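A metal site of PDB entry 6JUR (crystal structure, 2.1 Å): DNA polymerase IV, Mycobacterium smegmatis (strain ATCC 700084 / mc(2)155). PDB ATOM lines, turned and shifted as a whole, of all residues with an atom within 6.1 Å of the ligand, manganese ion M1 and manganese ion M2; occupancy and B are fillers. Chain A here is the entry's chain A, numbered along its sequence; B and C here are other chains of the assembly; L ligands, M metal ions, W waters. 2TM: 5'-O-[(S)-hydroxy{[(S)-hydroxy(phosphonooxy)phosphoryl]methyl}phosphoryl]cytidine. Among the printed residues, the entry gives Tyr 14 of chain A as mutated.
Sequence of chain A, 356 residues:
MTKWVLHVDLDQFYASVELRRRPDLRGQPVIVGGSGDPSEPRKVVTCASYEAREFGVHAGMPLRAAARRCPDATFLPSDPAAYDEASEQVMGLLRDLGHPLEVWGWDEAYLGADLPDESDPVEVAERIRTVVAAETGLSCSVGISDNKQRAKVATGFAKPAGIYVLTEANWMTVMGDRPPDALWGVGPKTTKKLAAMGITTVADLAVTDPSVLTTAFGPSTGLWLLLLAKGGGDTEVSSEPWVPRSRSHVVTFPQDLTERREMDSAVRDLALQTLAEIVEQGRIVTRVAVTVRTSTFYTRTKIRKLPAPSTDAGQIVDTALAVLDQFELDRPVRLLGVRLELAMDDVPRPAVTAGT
The side-chain amino group (NZ) of Lys 152 sits close to an oxygen (O1A) of the ligand (3.9 Å).
The guanidinium group (NH1) of Arg 53 is in salt-bridge range of an oxygen (O1G) of the ligand (2.5 Å).
N4 of DC 18 of chain C lies within hydrogen-bond range of a nitrogen (N4) of the ligand (3.3 Å).
O of Thr 46 lies within hydrogen-bond range of O2' of the ligand.
O6 of DG 4 of chain B lies within hydrogen-bond range of N4 of the ligand.
An oxygen (O2G) of the ligand lies close to the backbone NH (N) of Gln 12, 3.1 Å away.
The side-chain amino group of Lys 159 lies close to an oxygen (O2G) of the ligand, at 2.8 Å.
The backbone NH of Phe 13 lies close to an oxygen (O2B) of the ligand (3.1 Å).
The side-chain hydroxyl (OH) of Tyr 50 is in hydrogen-bond range of an oxygen (O1G) of the ligand (3.4 Å).
The side-chain amino group of Lys 159 is in salt-bridge range of the side-chain carboxylate of Asp 11 (2.7 Å).
N4 of DC 18 of chain C sits close to O6 of DG 5 of chain B (2.6 Å).
OE1 of Glu 108 lies within salt-bridge range of NZ of Lys 152, 2.9 Å away.
The side-chain amino group (NZ) of Lys 159 sits at hydrogen-bond distance from the backbone carbonyl oxygen (O) of Asp 9 (3.2 Å).
NE2 of His 7 sits at hydrogen-bond distance from OE1 of Glu 108 (2.7 Å).
The backbone carbonyl oxygen (O) of Leu 10 sits close to the side-chain amino group (NZ) of Lys 159, at 3.5 Å.
O of Ala 48 lies within hydrogen-bond range of NE of Arg 53 (2.9 Å).
OE1 of Gln 12 is in hydrogen-bond range of N of Tyr 50.
Merely in contact with the ligand: Asp 11 (3.6 Å), Tyr 14 (3.2 Å) and DG 5 of chain B (3.5 Å).
Hydrophobic or aromatic side chains within 4 Å of the ligand: Phe 13, Tyr 14 and Tyr 50.
16 residues have an atom within 4 Å of the ligand: Asp 9, Leu 10, Asp 11, Gln 12, Phe 13, Tyr 14, Thr 46, Tyr 50, Arg 53, Asp 107, Glu 108, Lys 152, Lys 159, DG 4 of chain B, DG 5 of chain B and DC 18 of chain C.
Along chain A the residues within 4 Å of the ligand span positions 9 to 159.
The nearest printed residue that does not touch the ligand is Ala 59 (4.3 Å).
Of the 22 residues printed, 3 come within 4 Å of manganese ion M1.
Lys 159 touches manganese ion M2 (NZ to MN, 3.6 Å).
Of the 22 residues printed, 4 come within 4 Å of manganese ion M2.
The nearest printed residue that does not touch manganese ion M2 is Gln 12 (4.2 Å).
Manganese ion M1 is bound by an oxygen (O1A) of the ligand, at 1.8 Å.
OD2 of Asp 9 binds manganese ion M1.
Manganese ion M1 is bound by OD2 of Asp 107, 2.4 Å away.
OE2 of Glu 108 binds manganese ion M1.
OD1 of Asp 107 binds manganese ion M1, 2.6 Å away.
Manganese ion M1 has five donor atoms within binding distance.
Manganese ion M2 is bound by OD2 of Asp 107, OD1 of Asp 9, O of Leu 10, O2B of the ligand and O2G of the ligand.
Manganese ion M2 has five donor atoms within binding distance.
Water W3 bridges an oxygen (O1G) of the ligand and the guanidinium group (NH1) of Arg 53.
Water W4 lies within hydrogen-bond range of an oxygen (O3') of the ligand, the backbone NH (N) of Tyr 14, the backbone NH (N) of Phe 13 and the side-chain sulfur (SG) of Cys 47.
Water W1 bridges an oxygen (O2) of the ligand and the side-chain hydroxyl of Tyr 14.
Water W2 lies within hydrogen-bond range of O2 of DC 18 of chain C and an oxygen (O4') of the ligand.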
ATOM      1  N   HIS A   7      -8.314  21.820  35.089  1.00  0.00           N
ATOM      2  CA  HIS A   7      -9.156  22.892  34.602  1.00  0.00           C
ATOM      3  C   HIS A   7     -10.541  22.203  34.493  1.00  0.00           C
ATOM      4  O   HIS A   7     -10.634  21.216  33.710  1.00  0.00           O
ATOM      5  CB  HIS A   7      -8.710  23.443  33.226  1.00  0.00           C
ATOM      6  CG  HIS A   7      -9.636  24.473  32.689  1.00  0.00           C
ATOM      7  ND1 HIS A   7     -10.500  24.193  31.646  1.00  0.00           N
ATOM      8  CD2 HIS A   7      -9.895  25.780  33.077  1.00  0.00           C
ATOM      9  CE1 HIS A   7     -11.290  25.248  31.445  1.00  0.00           C
ATOM     10  NE2 HIS A   7     -10.905  26.232  32.250  1.00  0.00           N
ATOM     11  N   ASP A   9     -14.488  22.459  33.457  1.00  0.00           N
ATOM     12  CA  ASP A   9     -15.250  23.356  32.623  1.00  0.00           C
ATOM     13  C   ASP A   9     -16.636  22.663  32.415  1.00  0.00           C
ATOM     14  O   ASP A   9     -16.701  21.580  31.845  1.00  0.00           O
ATOM     15  CB  ASP A   9     -14.506  23.494  31.314  1.00  0.00           C
ATOM     16  CG  ASP A   9     -15.237  24.492  30.323  1.00  0.00           C
ATOM     17  OD1 ASP A   9     -16.420  24.271  30.157  1.00  0.00           O
ATOM     18  OD2 ASP A   9     -14.773  25.596  29.822  1.00  0.00           O
ATOM     19  N   LEU A  10     -17.727  23.335  32.764  1.00  0.00           N
ATOM     20  CA  LEU A  10     -19.060  22.788  32.527  1.00  0.00           C
ATOM     21  C   LEU A  10     -19.475  22.693  31.068  1.00  0.00           C
ATOM     22  O   LEU A  10     -19.344  23.711  30.347  1.00  0.00           O
ATOM     23  CB  LEU A  10     -20.107  23.631  33.255  1.00  0.00           C
ATOM     24  CG  LEU A  10     -20.026  23.555  34.777  1.00  0.00           C
ATOM     25  CD1 LEU A  10     -20.568  24.810  35.465  1.00  0.00           C
ATOM     26  CD2 LEU A  10     -20.728  22.245  35.212  1.00  0.00           C
ATOM     27  N   ASP A  11     -19.964  21.549  30.625  1.00  0.00           N
ATOM     28  CA  ASP A  11     -20.181  21.333  29.178  1.00  0.00           C
ATOM     29  C   ASP A  11     -21.441  22.135  28.738  1.00  0.00           C
ATOM     30  O   ASP A  11     -22.409  22.174  29.504  1.00  0.00           O
ATOM     31  CB  ASP A  11     -20.430  19.867  28.942  1.00  0.00           C
ATOM     32  CG  ASP A  11     -19.176  19.020  29.197  1.00  0.00           C
ATOM     33  OD1 ASP A  11     -18.009  19.534  29.241  1.00  0.00           O
ATOM     34  OD2 ASP A  11     -19.331  17.789  29.260  1.00  0.00           O
ATOM     35  N   GLN A  12     -21.394  22.849  27.585  1.00  0.00           N
ATOM     36  CA  GLN A  12     -22.494  23.634  27.054  1.00  0.00           C
ATOM     37  C   GLN A  12     -23.325  24.243  28.183  1.00  0.00           C
ATOM     38  O   GLN A  12     -24.540  23.982  28.327  1.00  0.00           O
ATOM     39  CB  GLN A  12     -23.408  22.754  26.109  1.00  0.00           C
ATOM     40  CG  GLN A  12     -23.831  21.395  26.728  1.00  0.00           C
ATOM     41  CD  GLN A  12     -24.745  20.628  25.843  1.00  0.00           C
ATOM     42  OE1 GLN A  12     -25.093  21.074  24.728  1.00  0.00           O
ATOM     43  NE2 GLN A  12     -25.110  19.456  26.278  1.00  0.00           N
ATOM     44  N   PHE A  13     -22.629  25.067  28.981  1.00  0.00           N
ATOM     45  CA  PHE A  13     -23.155  25.397  30.289  1.00  0.00           C
ATOM     46  C   PHE A  13     -24.624  25.904  30.265  1.00  0.00           C
ATOM     47  O   PHE A  13     -25.440  25.334  30.927  1.00  0.00           O
ATOM     48  CB  PHE A  13     -22.277  26.479  30.975  1.00  0.00           C
ATOM     49  CG  PHE A  13     -22.755  26.883  32.360  1.00  0.00           C
ATOM     50  CD1 PHE A  13     -23.273  25.885  33.243  1.00  0.00           C
ATOM     51  CD2 PHE A  13     -22.651  28.196  32.787  1.00  0.00           C
ATOM     52  CE1 PHE A  13     -23.693  26.220  34.531  1.00  0.00           C
ATOM     53  CE2 PHE A  13     -23.077  28.526  34.081  1.00  0.00           C
ATOM     54  CZ  PHE A  13     -23.610  27.551  34.953  1.00  0.00           C
ATOM     55  N   TYR A  14     -24.895  27.032  29.576  1.00  0.00           N
ATOM     56  CA  TYR A  14     -26.281  27.570  29.644  1.00  0.00           C
ATOM     57  C   TYR A  14     -27.320  26.617  29.109  1.00  0.00           C
ATOM     58  O   TYR A  14     -28.414  26.540  29.642  1.00  0.00           O
ATOM     59  CB  TYR A  14     -26.409  28.889  28.913  1.00  0.00           C
ATOM     60  CG  TYR A  14     -25.509  30.048  29.391  1.00  0.00           C
ATOM     61  CD1 TYR A  14     -24.742  29.983  30.632  1.00  0.00           C
ATOM     62  CD2 TYR A  14     -25.478  31.244  28.626  1.00  0.00           C
ATOM     63  CE1 TYR A  14     -23.957  31.060  30.999  1.00  0.00           C
ATOM     64  CE2 TYR A  14     -24.674  32.253  29.020  1.00  0.00           C
ATOM     65  CZ  TYR A  14     -23.959  32.152  30.179  1.00  0.00           C
ATOM     66  OH  TYR A  14     -23.237  33.216  30.479  1.00  0.00           O
ATOM     67  N   VAL A  45     -26.419  34.329  19.759  1.00  0.00           N
ATOM     68  CA  VAL A  45     -26.521  33.092  20.546  1.00  0.00           C
ATOM     69  C   VAL A  45     -25.517  33.194  21.662  1.00  0.00           C
ATOM     70  O   VAL A  45     -24.405  33.604  21.460  1.00  0.00           O
ATOM     71  CB  VAL A  45     -26.138  31.908  19.615  1.00  0.00           C
ATOM     72  CG1 VAL A  45     -25.985  30.617  20.423  1.00  0.00           C
ATOM     73  CG2 VAL A  45     -27.204  31.818  18.476  1.00  0.00           C
ATOM     74  N   THR A  46     -25.934  32.793  22.877  1.00  0.00           N
ATOM     75  CA  THR A  46     -25.107  32.748  24.061  1.00  0.00           C
ATOM     76  C   THR A  46     -24.695  31.324  24.494  1.00  0.00           C
ATOM     77  O   THR A  46     -23.670  31.110  25.102  1.00  0.00           O
ATOM     78  CB  THR A  46     -26.023  33.444  25.104  1.00  0.00           C
ATOM     79  OG1 THR A  46     -25.206  33.995  26.022  1.00  0.00           O
ATOM     80  CG2 THR A  46     -26.929  32.594  25.742  1.00  0.00           C
ATOM     81  N   CYS A  47     -25.426  30.315  24.000  1.00  0.00           N
ATOM     82  CA  CYS A  47     -24.985  28.949  24.045  1.00  0.00           C
ATOM     83  C   CYS A  47     -25.808  28.121  23.075  1.00  0.00           C
ATOM     84  O   CYS A  47     -27.026  28.199  23.046  1.00  0.00           O
ATOM     85  CB  CYS A  47     -25.183  28.379  25.526  1.00  0.00           C
ATOM     86  SG  CYS A  47     -24.573  26.737  25.687  1.00  0.00           S
ATOM     87  N   ALA A  48     -25.129  27.349  22.212  1.00  0.00           N
ATOM     88  CA  ALA A  48     -25.834  26.360  21.398  1.00  0.00           C
ATOM     89  C   ALA A  48     -25.621  24.979  21.977  1.00  0.00           C
ATOM     90  O   ALA A  48     -24.502  24.636  22.190  1.00  0.00           O
ATOM     91  CB  ALA A  48     -25.301  26.419  19.945  1.00  0.00           C
ATOM     92  N   TYR A  50     -25.073  20.919  21.782  1.00  0.00           N
ATOM     93  CA  TYR A  50     -24.185  20.191  20.819  1.00  0.00           C
ATOM     94  C   TYR A  50     -24.921  19.870  19.530  1.00  0.00           C
ATOM     95  O   TYR A  50     -24.330  19.935  18.431  1.00  0.00           O
ATOM     96  CB  TYR A  50     -23.643  18.892  21.425  1.00  0.00           C
ATOM     97  CG  TYR A  50     -22.770  19.141  22.596  1.00  0.00           C
ATOM     98  CD1 TYR A  50     -21.878  20.187  22.555  1.00  0.00           C
ATOM     99  CD2 TYR A  50     -22.829  18.380  23.782  1.00  0.00           C
ATOM    100  CE1 TYR A  50     -21.025  20.491  23.612  1.00  0.00           C
ATOM    101  CE2 TYR A  50     -21.927  18.677  24.888  1.00  0.00           C
ATOM    102  CZ  TYR A  50     -21.041  19.742  24.786  1.00  0.00           C
ATOM    103  OH  TYR A  50     -20.032  20.156  25.805  1.00  0.00           O
ATOM    104  N   ARG A  53     -24.912  22.866  17.338  1.00  0.00           N
ATOM    105  CA  ARG A  53     -23.592  23.097  16.803  1.00  0.00           C
ATOM    106  C   ARG A  53     -23.322  22.203  15.576  1.00  0.00           C
ATOM    107  O   ARG A  53     -22.504  22.584  14.755  1.00  0.00           O
ATOM    108  CB  ARG A  53     -22.540  22.685  17.850  1.00  0.00           C
ATOM    109  CG  ARG A  53     -22.571  23.592  19.055  1.00  0.00           C
ATOM    110  CD  ARG A  53     -21.534  23.149  20.126  1.00  0.00           C
ATOM    111  NE  ARG A  53     -21.851  23.893  21.347  1.00  0.00           N
ATOM    112  CZ  ARG A  53     -21.043  24.056  22.427  1.00  0.00           C
ATOM    113  NH1 ARG A  53     -19.851  23.512  22.423  1.00  0.00           N
ATOM    114  NH2 ARG A  53     -21.487  24.725  23.494  1.00  0.00           N
ATOM    115  N   ALA A  59     -21.811  30.174  19.875  1.00  0.00           N
ATOM    116  CA  ALA A  59     -21.912  31.408  20.705  1.00  0.00           C
ATOM    117  C   ALA A  59     -21.259  32.537  19.950  1.00  0.00           C
ATOM    118  O   ALA A  59     -20.225  32.346  19.308  1.00  0.00           O
ATOM    119  CB  ALA A  59     -21.232  31.245  22.059  1.00  0.00           C
ATOM    120  N   GLY A  60     -21.919  33.673  19.873  1.00  0.00           N
ATOM    121  CA  GLY A  60     -21.355  34.731  19.069  1.00  0.00           C
ATOM    122  C   GLY A  60     -22.082  34.872  17.786  1.00  0.00           C
ATOM    123  O   GLY A  60     -22.176  35.992  17.260  1.00  0.00           O
ATOM    124  N   ASP A 107     -18.486  29.329  33.850  1.00  0.00           N
ATOM    125  CA  ASP A 107     -18.443  27.882  33.641  1.00  0.00           C
ATOM    126  C   ASP A 107     -17.141  27.127  33.919  1.00  0.00           C
ATOM    127  O   ASP A 107     -17.100  25.924  33.663  1.00  0.00           O
ATOM    128  CB  ASP A 107     -18.962  27.497  32.297  1.00  0.00           C
ATOM    129  CG  ASP A 107     -17.937  27.674  31.210  1.00  0.00           C
ATOM    130  OD1 ASP A 107     -17.170  28.663  31.242  1.00  0.00           O
ATOM    131  OD2 ASP A 107     -17.946  26.883  30.247  1.00  0.00           O
ATOM    132  N   GLU A 108     -16.132  27.786  34.523  1.00  0.00           N
ATOM    133  CA  GLU A 108     -14.823  27.187  34.635  1.00  0.00           C
ATOM    134  C   GLU A 108     -14.195  27.572  35.885  1.00  0.00           C
ATOM    135  O   GLU A 108     -14.369  28.692  36.344  1.00  0.00           O
ATOM    136  CB  GLU A 108     -13.830  27.778  33.588  1.00  0.00           C
ATOM    137  CG  GLU A 108     -14.284  27.601  32.183  1.00  0.00           C
ATOM    138  CD  GLU A 108     -13.432  28.375  31.163  1.00  0.00           C
ATOM    139  OE1 GLU A 108     -12.197  28.434  31.351  1.00  0.00           O
ATOM    140  OE2 GLU A 108     -14.041  28.819  30.165  1.00  0.00           O
ATOM    141  N   LYS A 152      -6.031  24.082  30.263  1.00  0.00           N
ATOM    142  CA  LYS A 152      -7.146  24.604  29.537  1.00  0.00           C
ATOM    143  C   LYS A 152      -7.119  24.034  28.119  1.00  0.00           C
ATOM    144  O   LYS A 152      -8.141  23.700  27.578  1.00  0.00           O
ATOM    145  CB  LYS A 152      -6.987  26.178  29.538  1.00  0.00           C
ATOM    146  CG  LYS A 152      -7.914  26.817  28.502  1.00  0.00           C
ATOM    147  CD  LYS A 152      -9.343  26.928  29.042  1.00  0.00           C
ATOM    148  CE  LYS A 152     -10.239  27.745  28.060  1.00  0.00           C
ATOM    149  NZ  LYS A 152     -11.661  27.771  28.538  1.00  0.00           N
ATOM    150  N   LYS A 159     -13.513  17.536  26.207  1.00  0.00           N
ATOM    151  CA  LYS A 159     -14.904  17.671  25.906  1.00  0.00           C
ATOM    152  C   LYS A 159     -15.344  16.611  24.846  1.00  0.00           C
ATOM    153  O   LYS A 159     -14.564  16.287  23.954  1.00  0.00           O
ATOM    154  CB  LYS A 159     -15.252  19.024  25.343  1.00  0.00           C
ATOM    155  CG  LYS A 159     -14.762  20.275  26.141  1.00  0.00           C
ATOM    156  CD  LYS A 159     -15.812  20.689  27.089  1.00  0.00           C
ATOM    157  CE  LYS A 159     -15.642  22.030  27.752  1.00  0.00           C
ATOM    158  NZ  LYS A 159     -16.865  21.966  28.669  1.00  0.00           N
ATOM    159  P    DG B   4     -22.775  42.884  17.534  1.00  0.00           P
ATOM    160  OP1  DG B   4     -23.534  44.108  17.229  1.00  0.00           O
ATOM    161  OP2  DG B   4     -21.341  42.978  17.828  1.00  0.00           O
ATOM    162  O5'  DG B   4     -23.430  42.196  18.784  1.00  0.00           O
ATOM    163  C5'  DG B   4     -24.857  42.065  18.888  1.00  0.00           C
ATOM    164  C4'  DG B   4     -25.151  41.957  20.366  1.00  0.00           C
ATOM    165  O4'  DG B   4     -24.718  40.687  20.929  1.00  0.00           O
ATOM    166  C3'  DG B   4     -24.470  43.065  21.165  1.00  0.00           C
ATOM    167  O3'  DG B   4     -25.393  43.442  22.166  1.00  0.00           O
ATOM    168  C2'  DG B   4     -23.299  42.406  21.872  1.00  0.00           C
ATOM    169  C1'  DG B   4     -23.657  40.905  21.880  1.00  0.00           C
ATOM    170  N9   DG B   4     -22.547  40.066  21.472  1.00  0.00           N
ATOM    171  C8   DG B   4     -21.863  40.114  20.279  1.00  0.00           C
ATOM    172  N7   DG B   4     -20.919  39.226  20.184  1.00  0.00           N
ATOM    173  C5   DG B   4     -20.998  38.521  21.385  1.00  0.00           C
ATOM    174  C6   DG B   4     -20.226  37.435  21.867  1.00  0.00           C
ATOM    175  O6   DG B   4     -19.289  36.849  21.316  1.00  0.00           O
ATOM    176  N1   DG B   4     -20.577  37.091  23.181  1.00  0.00           N
ATOM    177  C2   DG B   4     -21.604  37.661  23.889  1.00  0.00           C
ATOM    178  N2   DG B   4     -21.838  37.127  25.086  1.00  0.00           N
ATOM    179  N3   DG B   4     -22.363  38.652  23.435  1.00  0.00           N
ATOM    180  C4   DG B   4     -21.987  39.052  22.191  1.00  0.00           C
ATOM    181  P    DG B   5     -24.987  44.623  23.221  1.00  0.00           P
ATOM    182  OP1  DG B   5     -26.281  45.193  23.671  1.00  0.00           O
ATOM    183  OP2  DG B   5     -23.971  45.501  22.592  1.00  0.00           O
ATOM    184  O5'  DG B   5     -24.338  43.823  24.451  1.00  0.00           O
ATOM    185  C5'  DG B   5     -25.127  42.927  25.234  1.00  0.00           C
ATOM    186  C4'  DG B   5     -24.273  42.424  26.364  1.00  0.00           C
ATOM    187  O4'  DG B   5     -23.280  41.509  25.833  1.00  0.00           O
ATOM    188  C3'  DG B   5     -23.469  43.579  27.021  1.00  0.00           C
ATOM    189  O3'  DG B   5     -23.591  43.291  28.400  1.00  0.00           O
ATOM    190  C2'  DG B   5     -22.015  43.331  26.591  1.00  0.00           C
ATOM    191  C1'  DG B   5     -22.014  41.806  26.381  1.00  0.00           C
ATOM    192  N9   DG B   5     -20.980  41.310  25.479  1.00  0.00           N
ATOM    193  C8   DG B   5     -20.586  41.846  24.267  1.00  0.00           C
ATOM    194  N7   DG B   5     -19.597  41.192  23.724  1.00  0.00           N
ATOM    195  C5   DG B   5     -19.300  40.173  24.631  1.00  0.00           C
ATOM    196  C6   DG B   5     -18.324  39.129  24.578  1.00  0.00           C
ATOM    197  O6   DG B   5     -17.496  38.881  23.692  1.00  0.00           O
ATOM    198  N1   DG B   5     -18.433  38.280  25.687  1.00  0.00           N
ATOM    199  C2   DG B   5     -19.315  38.433  26.726  1.00  0.00           C
ATOM    200  N2   DG B   5     -19.231  37.529  27.706  1.00  0.00           N
ATOM    201  N3   DG B   5     -20.236  39.385  26.766  1.00  0.00           N
ATOM    202  C4   DG B   5     -20.151  40.235  25.723  1.00  0.00           C
ATOM    203  P    DC C  18     -10.810  31.596  27.807  1.00  0.00           P
ATOM    204  OP1  DC C  18     -10.155  30.730  28.808  1.00  0.00           O
ATOM    205  OP2  DC C  18     -11.150  31.139  26.374  1.00  0.00           O
ATOM    206  O5'  DC C  18     -12.245  32.093  28.370  1.00  0.00           O
ATOM    207  C5'  DC C  18     -12.504  32.491  29.707  1.00  0.00           C
ATOM    208  C4'  DC C  18     -13.999  32.749  29.784  1.00  0.00           C
ATOM    209  O4'  DC C  18     -14.362  33.897  28.990  1.00  0.00           O
ATOM    210  C3'  DC C  18     -14.913  31.600  29.321  1.00  0.00           C
ATOM    211  O3'  DC C  18     -15.755  31.320  30.422  1.00  0.00           O
ATOM    212  C2'  DC C  18     -15.569  32.125  28.056  1.00  0.00           C
ATOM    213  C1'  DC C  18     -15.560  33.623  28.322  1.00  0.00           C
ATOM    214  N1   DC C  18     -15.571  34.494  27.151  1.00  0.00           N
ATOM    215  C2   DC C  18     -16.565  35.490  27.058  1.00  0.00           C
ATOM    216  O2   DC C  18     -17.439  35.529  27.915  1.00  0.00           O
ATOM    217  N3   DC C  18     -16.604  36.277  25.972  1.00  0.00           N
ATOM    218  C4   DC C  18     -15.679  36.149  25.009  1.00  0.00           C
ATOM    219  N4   DC C  18     -15.746  36.966  23.957  1.00  0.00           N
ATOM    220  C5   DC C  18     -14.625  35.176  25.103  1.00  0.00           C
ATOM    221  C6   DC C  18     -14.613  34.380  26.185  1.00  0.00           C
HETATM  222  O5' 2TM L   1     -18.005  28.812  27.108  1.00  0.00           O
HETATM  223  C5' 2TM L   1     -18.061  30.156  27.231  1.00  0.00           C
HETATM  224  C4' 2TM L   1     -19.419  30.639  27.702  1.00  0.00           C
HETATM  225  O4' 2TM L   1     -19.155  32.046  27.728  1.00  0.00           O
HETATM  226  C3' 2TM L   1     -20.287  30.431  26.504  1.00  0.00           C
HETATM  227  O3' 2TM L   1     -21.141  29.322  26.469  1.00  0.00           O
HETATM  228  C2' 2TM L   1     -20.974  31.723  26.280  1.00  0.00           C
HETATM  229  O2' 2TM L   1     -22.147  31.758  27.079  1.00  0.00           O
HETATM  230  C1' 2TM L   1     -20.011  32.740  26.886  1.00  0.00           C
HETATM  231  C5  2TM L   1     -17.816  33.265  23.945  1.00  0.00           C
HETATM  232  C6  2TM L   1     -18.313  32.710  25.073  1.00  0.00           C
HETATM  233  N1  2TM L   1     -19.382  33.271  25.723  1.00  0.00           N
HETATM  234  C2  2TM L   1     -19.932  34.442  25.274  1.00  0.00           C
HETATM  235  N3  2TM L   1     -19.456  35.013  24.212  1.00  0.00           N
HETATM  236  C4  2TM L   1     -18.406  34.404  23.545  1.00  0.00           C
HETATM  237  O3G 2TM L   1     -17.089  24.848  25.119  1.00  0.00           O
HETATM  238  PG  2TM L   1     -18.362  24.088  25.568  1.00  0.00           P
HETATM  239  O1G 2TM L   1     -18.669  23.033  24.576  1.00  0.00           O
HETATM  240  O2G 2TM L   1     -18.431  23.544  26.967  1.00  0.00           O
HETATM  241  O3B 2TM L   1     -19.515  25.054  25.500  1.00  0.00           O
HETATM  242  PB  2TM L   1     -19.271  26.555  26.213  1.00  0.00           P
HETATM  243  O1B 2TM L   1     -19.889  27.468  25.154  1.00  0.00           O
HETATM  244  O2B 2TM L   1     -20.040  26.259  27.680  1.00  0.00           O
HETATM  245  PA  2TM L   1     -16.699  28.016  27.179  1.00  0.00           P
HETATM  246  O1A 2TM L   1     -15.484  28.294  28.113  1.00  0.00           O
HETATM  247  O2A 2TM L   1     -16.141  28.792  25.572  1.00  0.00           O
HETATM  248  N4  2TM L   1     -17.864  34.975  22.488  1.00  0.00           N
HETATM  249  O2  2TM L   1     -20.878  34.968  25.882  1.00  0.00           O
HETATM  250  C1  2TM L   1     -17.490  26.768  26.310  1.00  0.00           C
HETATM  251 MN    MN M   1     -15.717  27.254  29.584  1.00  0.00          MN
HETATM  252 MN    MN M   2     -18.203  25.273  28.978  1.00  0.00          MN
HETATM  253  O   HOH W   1     -22.334  34.906  28.275  1.00  0.00           O
HETATM  254  O   HOH W   2     -19.101  34.556  29.806  1.00  0.00           O
HETATM  255  O   HOH W   3     -16.776  22.469  23.011  1.00  0.00           O
HETATM  256  O   HOH W   4     -22.753  28.192  28.201  1.00  0.00           O
